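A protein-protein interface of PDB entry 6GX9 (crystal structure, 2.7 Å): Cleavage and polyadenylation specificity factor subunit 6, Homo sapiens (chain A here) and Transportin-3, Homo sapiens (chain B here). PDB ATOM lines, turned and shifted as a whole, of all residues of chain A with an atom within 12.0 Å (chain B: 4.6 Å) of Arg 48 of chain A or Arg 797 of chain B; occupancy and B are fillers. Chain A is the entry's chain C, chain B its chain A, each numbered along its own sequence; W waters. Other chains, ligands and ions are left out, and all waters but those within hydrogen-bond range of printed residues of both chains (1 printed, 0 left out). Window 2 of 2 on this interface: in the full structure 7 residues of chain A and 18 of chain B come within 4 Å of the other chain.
O3P of SEP 45 of chain A sits close to the guanidinium group (NH2) of Arg 671 of chain B, at 3.0 Å. OD2 of Asp 709 of chain B is in salt-bridge range of NH2 of Arg 48 of chain A (3.2 Å). NH2 of Arg 758 of chain B sits close to O2P of SEP 45 of chain A (3.1 Å). OE2 of Glu 47 of chain A is in hydrogen-bond range of SG of Cys 793 of chain B, 3.2 Å away. The side-chain carboxylate (OE1) of Glu 47 of chain A lies within salt-bridge range of the guanidinium group (NH1) of Arg 797 of chain B (3.9 Å). The guanidinium group (NH2) of Arg 797 of chain B is in hydrogen-bond range of the backbone carbonyl oxygen (O) of Arg 48 of chain A (3.4 Å). The guanidinium group of Arg 48 of chain A sits close to the guanidinium group of Arg 758 of chain B (3.2 Å).
The guanidinium group of Arg 671 of chain B lies within salt-bridge range of the side-chain carboxylate of Asp 709 of chain B (2.6 Å). The side-chain carboxylate of Asp 709 of chain B is in salt-bridge range of the guanidinium group of Arg 758 of chain B (3.99 Å). NH1 of Arg 758 of chain B lies close to NE2 of Gln 761 of chain B (3.3 Å). The guanidinium group (NH2) of Arg 48 of chain A sits close to O1P of SEP 45 of chain A, 2.6 Å away.
Arg 48 of chain A touches Arg 671 of chain B.
Arg 48 of chain A touches just these residues of chain B: Arg 671, Asp 709, Arg 758 and Arg 797. Asp 709 of chain B touches just one residue of chain A: Arg 48 (3.2 Å). No residue of chain A comes within 4 Å of Thr 757 of chain B. Cys 793 of chain B touches one residue of chain A. No residue of chain A comes within 4 Å of Val 795 of chain B. No residue of chain A comes within 4 Å of Phe 798 of chain B. Printed residues of chain A within 4 Å of Arg 758 of chain B: SEP 45 and Arg 48. Of the printed residues of chain B, Glu 47 of chain A touches Cys 793 (3.2 Å) and Arg 797 (3.7 Å). Of the printed residues of chain A, Arg 671 of chain B touches SEP 45 (3.0 Å) and Arg 48 (3.5 Å). Arg 46 of chain A touches none of the printed residues of chain B.
Of the 6 printed residues of chain A, 3 touch a printed residue of chain B. Among the printed residues, 8 pairs touch across the chains. Among the printed residues, Asp or Glu carboxylates within 4 Å of a Lys or Arg side-chain nitrogen of the other chain: Glu 47 of chain A with Arg 797 of chain B (3.9 Å) and Arg 48 of chain A with Asp 709 of chain B (3.2 Å).
Water W1 lies within hydrogen-bond range of the guanidinium group of Arg 671 of chain B (2.6 Å) and O3P of SEP 45 of chain A (2.7 Å).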
ATOM      1  N   GLU A  43      -1.448 -19.568  11.077  1.00  0.00           N
ATOM      2  CA  GLU A  43      -2.643 -20.222  11.592  1.00  0.00           C
ATOM      3  C   GLU A  43      -3.666 -19.170  11.996  1.00  0.00           C
ATOM      4  O   GLU A  43      -3.348 -18.245  12.749  1.00  0.00           O
ATOM      5  CB  GLU A  43      -2.313 -21.130  12.782  1.00  0.00           C
ATOM      6  CG  GLU A  43      -3.494 -21.967  13.252  1.00  0.00           C
ATOM      7  CD  GLU A  43      -3.272 -22.574  14.620  1.00  0.00           C
ATOM      8  OE1 GLU A  43      -2.160 -23.085  14.867  1.00  0.00           O
ATOM      9  OE2 GLU A  43      -4.209 -22.541  15.447  1.00  0.00           O
ATOM     10  N   ARG A  44      -4.887 -19.314  11.489  1.00  0.00           N
ATOM     11  CA  ARG A  44      -5.990 -18.426  11.842  1.00  0.00           C
ATOM     12  C   ARG A  44      -7.115 -19.200  12.528  1.00  0.00           C
ATOM     13  O   ARG A  44      -7.147 -20.430  12.488  1.00  0.00           O
ATOM     14  CB  ARG A  44      -6.529 -17.717  10.598  1.00  0.00           C
ATOM     15  CG  ARG A  44      -5.535 -16.794   9.917  1.00  0.00           C
ATOM     16  CD  ARG A  44      -5.259 -15.572  10.774  1.00  0.00           C
ATOM     17  NE  ARG A  44      -4.234 -14.708  10.196  1.00  0.00           N
ATOM     18  CZ  ARG A  44      -2.938 -14.806  10.469  1.00  0.00           C
ATOM     19  NH1 ARG A  44      -2.509 -15.735  11.313  1.00  0.00           N
ATOM     20  NH2 ARG A  44      -2.072 -13.976   9.902  1.00  0.00           N
ATOM     21  N   SEP A  45      -8.037 -18.476  13.156  1.00  0.00           N
ATOM     22  CA  SEP A  45      -9.207 -19.100  13.767  1.00  0.00           C
ATOM     23  CB  SEP A  45      -9.766 -18.222  14.891  1.00  0.00           C
ATOM     24  OG  SEP A  45     -10.131 -16.934  14.416  1.00  0.00           O
ATOM     25  C   SEP A  45     -10.275 -19.366  12.707  1.00  0.00           C
ATOM     26  O   SEP A  45     -10.355 -18.656  11.704  1.00  0.00           O
ATOM     27  P   SEP A  45     -10.528 -15.977  15.652  1.00  0.00           P
ATOM     28  O1P SEP A  45     -11.811 -16.584  16.412  1.00  0.00           O
ATOM     29  O2P SEP A  45     -10.860 -14.499  15.110  1.00  0.00           O
ATOM     30  O3P SEP A  45      -9.298 -15.906  16.686  1.00  0.00           O
ATOM     31  N   ARG A  46     -11.089 -20.393  12.928  1.00  0.00           N
ATOM     32  CA  ARG A  46     -12.114 -20.778  11.961  1.00  0.00           C
ATOM     33  C   ARG A  46     -13.343 -19.876  12.059  1.00  0.00           C
ATOM     34  O   ARG A  46     -13.381 -18.944  12.864  1.00  0.00           O
ATOM     35  CB  ARG A  46     -12.520 -22.238  12.163  1.00  0.00           C
ATOM     36  N   GLU A  47     -14.347 -20.165  11.233  1.00  0.00           N
ATOM     37  CA  GLU A  47     -15.571 -19.380  11.218  1.00  0.00           C
ATOM     38  C   GLU A  47     -16.404 -19.660  12.468  1.00  0.00           C
ATOM     39  O   GLU A  47     -16.116 -20.564  13.257  1.00  0.00           O
ATOM     40  CB  GLU A  47     -16.386 -19.682   9.962  1.00  0.00           C
ATOM     41  CG  GLU A  47     -15.665 -19.383   8.661  1.00  0.00           C
ATOM     42  CD  GLU A  47     -16.496 -19.743   7.444  1.00  0.00           C
ATOM     43  OE1 GLU A  47     -17.591 -20.316   7.622  1.00  0.00           O
ATOM     44  OE2 GLU A  47     -16.056 -19.452   6.313  1.00  0.00           O
ATOM     45  N   ARG A  48     -17.466 -18.874  12.631  1.00  0.00           N
ATOM     46  CA  ARG A  48     -18.335 -18.985  13.800  1.00  0.00           C
ATOM     47  C   ARG A  48     -19.803 -19.077  13.395  1.00  0.00           C
ATOM     48  O   ARG A  48     -20.122 -19.360  12.241  1.00  0.00           O
ATOM     49  CB  ARG A  48     -18.126 -17.791  14.735  1.00  0.00           C
ATOM     50  CG  ARG A  48     -16.698 -17.622  15.226  1.00  0.00           C
ATOM     51  CD  ARG A  48     -16.539 -16.342  16.028  1.00  0.00           C
ATOM     52  NE  ARG A  48     -15.169 -16.149  16.494  1.00  0.00           N
ATOM     53  CZ  ARG A  48     -14.780 -15.136  17.262  1.00  0.00           C
ATOM     54  NH1 ARG A  48     -15.659 -14.221  17.651  1.00  0.00           N
ATOM     55  NH2 ARG A  48     -13.514 -15.036  17.643  1.00  0.00           N
ATOM     56  N   ARG B 671      -6.540 -14.524  24.684  1.00  0.00           N
ATOM     57  CA  ARG B 671      -7.752 -15.339  24.729  1.00  0.00           C
ATOM     58  C   ARG B 671      -7.922 -16.007  26.087  1.00  0.00           C
ATOM     59  O   ARG B 671      -9.036 -16.078  26.621  1.00  0.00           O
ATOM     60  CB  ARG B 671      -7.717 -16.397  23.625  1.00  0.00           C
ATOM     61  CG  ARG B 671      -7.772 -15.851  22.210  1.00  0.00           C
ATOM     62  CD  ARG B 671      -9.086 -15.145  21.936  1.00  0.00           C
ATOM     63  NE  ARG B 671      -9.263 -14.868  20.514  1.00  0.00           N
ATOM     64  CZ  ARG B 671     -10.263 -14.151  20.015  1.00  0.00           C
ATOM     65  NH1 ARG B 671     -11.175 -13.630  20.824  1.00  0.00           N
ATOM     66  NH2 ARG B 671     -10.350 -13.953  18.707  1.00  0.00           N
ATOM     67  N   ASP B 709     -11.879  -8.061  19.429  1.00  0.00           N
ATOM     68  CA  ASP B 709     -12.877  -9.058  19.799  1.00  0.00           C
ATOM     69  C   ASP B 709     -12.977  -9.220  21.310  1.00  0.00           C
ATOM     70  O   ASP B 709     -14.047  -9.566  21.825  1.00  0.00           O
ATOM     71  CB  ASP B 709     -12.550 -10.398  19.133  1.00  0.00           C
ATOM     72  CG  ASP B 709     -13.650 -11.433  19.319  1.00  0.00           C
ATOM     73  OD1 ASP B 709     -14.832 -11.112  19.068  1.00  0.00           O
ATOM     74  OD2 ASP B 709     -13.327 -12.574  19.708  1.00  0.00           O
ATOM     75  N   THR B 757     -14.211  -6.868  10.557  1.00  0.00           N
ATOM     76  CA  THR B 757     -15.379  -7.642  10.967  1.00  0.00           C
ATOM     77  C   THR B 757     -15.525  -7.646  12.484  1.00  0.00           C
ATOM     78  O   THR B 757     -16.618  -7.414  13.013  1.00  0.00           O
ATOM     79  CB  THR B 757     -15.281  -9.072  10.435  1.00  0.00           C
ATOM     80  OG1 THR B 757     -15.261  -9.046   9.003  1.00  0.00           O
ATOM     81  CG2 THR B 757     -16.462  -9.908  10.913  1.00  0.00           C
ATOM     82  N   ARG B 758     -14.430  -7.918  13.201  1.00  0.00           N
ATOM     83  CA  ARG B 758     -14.478  -7.879  14.657  1.00  0.00           C
ATOM     84  C   ARG B 758     -14.843  -6.493  15.163  1.00  0.00           C
ATOM     85  O   ARG B 758     -15.479  -6.362  16.215  1.00  0.00           O
ATOM     86  CB  ARG B 758     -13.135  -8.326  15.240  1.00  0.00           C
ATOM     87  CG  ARG B 758     -12.804  -9.783  14.967  1.00  0.00           C
ATOM     88  CD  ARG B 758     -13.759 -10.708  15.707  1.00  0.00           C
ATOM     89  NE  ARG B 758     -13.470 -12.116  15.451  1.00  0.00           N
ATOM     90  CZ  ARG B 758     -14.155 -12.876  14.602  1.00  0.00           C
ATOM     91  NH1 ARG B 758     -15.178 -12.366  13.930  1.00  0.00           N
ATOM     92  NH2 ARG B 758     -13.821 -14.148  14.427  1.00  0.00           N
ATOM     93  N   GLN B 761     -18.757  -5.803  14.722  1.00  0.00           N
ATOM     94  CA  GLN B 761     -19.632  -6.605  15.564  1.00  0.00           C
ATOM     95  C   GLN B 761     -19.429  -6.367  17.054  1.00  0.00           C
ATOM     96  O   GLN B 761     -20.287  -6.768  17.848  1.00  0.00           O
ATOM     97  CB  GLN B 761     -19.451  -8.101  15.256  1.00  0.00           C
ATOM     98  CG  GLN B 761     -18.072  -8.657  15.563  1.00  0.00           C
ATOM     99  CD  GLN B 761     -17.881 -10.071  15.032  1.00  0.00           C
ATOM    100  OE1 GLN B 761     -18.199 -10.364  13.877  1.00  0.00           O
ATOM    101  NE2 GLN B 761     -17.365 -10.956  15.880  1.00  0.00           N
ATOM    102  N   CYS B 793     -13.454 -14.833   1.480  1.00  0.00           N
ATOM    103  CA  CYS B 793     -14.342 -15.196   2.580  1.00  0.00           C
ATOM    104  C   CYS B 793     -14.360 -14.115   3.653  1.00  0.00           C
ATOM    105  O   CYS B 793     -15.410 -13.829   4.242  1.00  0.00           O
ATOM    106  CB  CYS B 793     -13.915 -16.536   3.181  1.00  0.00           C
ATOM    107  SG  CYS B 793     -14.817 -17.019   4.676  1.00  0.00           S
ATOM    108  N   SER B 794     -13.211 -13.485   3.900  1.00  0.00           N
ATOM    109  CA  SER B 794     -13.138 -12.456   4.930  1.00  0.00           C
ATOM    110  C   SER B 794     -13.848 -11.181   4.490  1.00  0.00           C
ATOM    111  O   SER B 794     -14.519 -10.527   5.297  1.00  0.00           O
ATOM    112  CB  SER B 794     -11.678 -12.168   5.273  1.00  0.00           C
ATOM    113  OG  SER B 794     -11.579 -11.285   6.374  1.00  0.00           O
ATOM    114  N   VAL B 795     -13.712 -10.814   3.213  1.00  0.00           N
ATOM    115  CA  VAL B 795     -14.353  -9.602   2.707  1.00  0.00           C
ATOM    116  C   VAL B 795     -15.868  -9.762   2.704  1.00  0.00           C
ATOM    117  O   VAL B 795     -16.604  -8.865   3.132  1.00  0.00           O
ATOM    118  CB  VAL B 795     -13.821  -9.262   1.303  1.00  0.00           C
ATOM    119  CG1 VAL B 795     -14.543  -8.054   0.739  1.00  0.00           C
ATOM    120  CG2 VAL B 795     -12.329  -9.005   1.354  1.00  0.00           C
ATOM    121  N   MET B 796     -16.358 -10.906   2.214  1.00  0.00           N
ATOM    122  CA  MET B 796     -17.799 -11.129   2.175  1.00  0.00           C
ATOM    123  C   MET B 796     -18.387 -11.195   3.577  1.00  0.00           C
ATOM    124  O   MET B 796     -19.508 -10.730   3.809  1.00  0.00           O
ATOM    125  CB  MET B 796     -18.113 -12.411   1.404  1.00  0.00           C
ATOM    126  CG  MET B 796     -17.677 -12.384  -0.049  1.00  0.00           C
ATOM    127  SD  MET B 796     -18.446 -11.053  -0.987  1.00  0.00           S
ATOM    128  CE  MET B 796     -17.643 -11.255  -2.576  1.00  0.00           C
ATOM    129  N   ARG B 797     -17.639 -11.762   4.527  1.00  0.00           N
ATOM    130  CA  ARG B 797     -18.106 -11.818   5.907  1.00  0.00           C
ATOM    131  C   ARG B 797     -18.221 -10.419   6.502  1.00  0.00           C
ATOM    132  O   ARG B 797     -19.141 -10.141   7.280  1.00  0.00           O
ATOM    133  CB  ARG B 797     -17.161 -12.688   6.736  1.00  0.00           C
ATOM    134  CG  ARG B 797     -17.685 -13.065   8.109  1.00  0.00           C
ATOM    135  CD  ARG B 797     -18.932 -13.926   7.983  1.00  0.00           C
ATOM    136  NE  ARG B 797     -19.206 -14.692   9.196  1.00  0.00           N
ATOM    137  CZ  ARG B 797     -18.814 -15.948   9.389  1.00  0.00           C
ATOM    138  NH1 ARG B 797     -18.129 -16.582   8.445  1.00  0.00           N
ATOM    139  NH2 ARG B 797     -19.110 -16.572  10.521  1.00  0.00           N
ATOM    140  N   PHE B 798     -17.302  -9.522   6.137  1.00  0.00           N
ATOM    141  CA  PHE B 798     -17.371  -8.148   6.620  1.00  0.00           C
ATOM    142  C   PHE B 798     -18.584  -7.423   6.051  1.00  0.00           C
ATOM    143  O   PHE B 798     -19.346  -6.792   6.792  1.00  0.00           O
ATOM    144  CB  PHE B 798     -16.088  -7.403   6.261  1.00  0.00           C
ATOM    145  CG  PHE B 798     -16.187  -5.916   6.426  1.00  0.00           C
ATOM    146  CD1 PHE B 798     -16.241  -5.347   7.689  1.00  0.00           C
ATOM    147  CD2 PHE B 798     -16.230  -5.086   5.319  1.00  0.00           C
ATOM    148  CE1 PHE B 798     -16.335  -3.978   7.842  1.00  0.00           C
ATOM    149  CE2 PHE B 798     -16.324  -3.714   5.465  1.00  0.00           C
ATOM    150  CZ  PHE B 798     -16.375  -3.159   6.729  1.00  0.00           C
ATOM    151  N   LEU B 799     -18.782  -7.506   4.732  1.00  0.00           N
ATOM    152  CA  LEU B 799     -19.938  -6.862   4.114  1.00  0.00           C
ATOM    153  C   LEU B 799     -21.241  -7.407   4.682  1.00  0.00           C
ATOM    154  O   LEU B 799     -22.205  -6.657   4.874  1.00  0.00           O
ATOM    155  CB  LEU B 799     -19.900  -7.048   2.596  1.00  0.00           C
ATOM    156  CG  LEU B 799     -18.737  -6.398   1.845  1.00  0.00           C
ATOM    157  CD1 LEU B 799     -18.726  -6.834   0.389  1.00  0.00           C
ATOM    158  CD2 LEU B 799     -18.811  -4.882   1.951  1.00  0.00           C
ATOM    159  N   ARG B 800     -21.285  -8.710   4.969  1.00  0.00           N
ATOM    160  CA  ARG B 800     -22.501  -9.310   5.509  1.00  0.00           C
ATOM    161  C   ARG B 800     -22.826  -8.748   6.888  1.00  0.00           C
ATOM    162  O   ARG B 800     -23.968  -8.364   7.163  1.00  0.00           O
ATOM    163  CB  ARG B 800     -22.349 -10.827   5.583  1.00  0.00           C
ATOM    164  CG  ARG B 800     -23.606 -11.542   6.032  1.00  0.00           C
ATOM    165  CD  ARG B 800     -23.284 -12.914   6.581  1.00  0.00           C
ATOM    166  NE  ARG B 800     -22.751 -12.828   7.938  1.00  0.00           N
ATOM    167  CZ  ARG B 800     -22.344 -13.871   8.652  1.00  0.00           C
ATOM    168  NH1 ARG B 800     -22.403 -15.094   8.139  1.00  0.00           N
ATOM    169  NH2 ARG B 800     -21.877 -13.692   9.881  1.00  0.00           N
ATOM    170  N   ASP B 801     -21.828  -8.695   7.773  1.00  0.00           N
ATOM    171  CA  ASP B 801     -22.069  -8.222   9.130  1.00  0.00           C
ATOM    172  C   ASP B 801     -22.226  -6.709   9.191  1.00  0.00           C
ATOM    173  O   ASP B 801     -22.923  -6.202  10.075  1.00  0.00           O
ATOM    174  CB  ASP B 801     -20.936  -8.676  10.051  1.00  0.00           C
ATOM    175  CG  ASP B 801     -20.976 -10.165  10.331  1.00  0.00           C
ATOM    176  OD1 ASP B 801     -22.073 -10.759  10.238  1.00  0.00           O
ATOM    177  OD2 ASP B 801     -19.914 -10.742  10.647  1.00  0.00           O
HETATM  178  O   HOH W   1      -8.248 -16.760  19.051  1.00  0.00           O
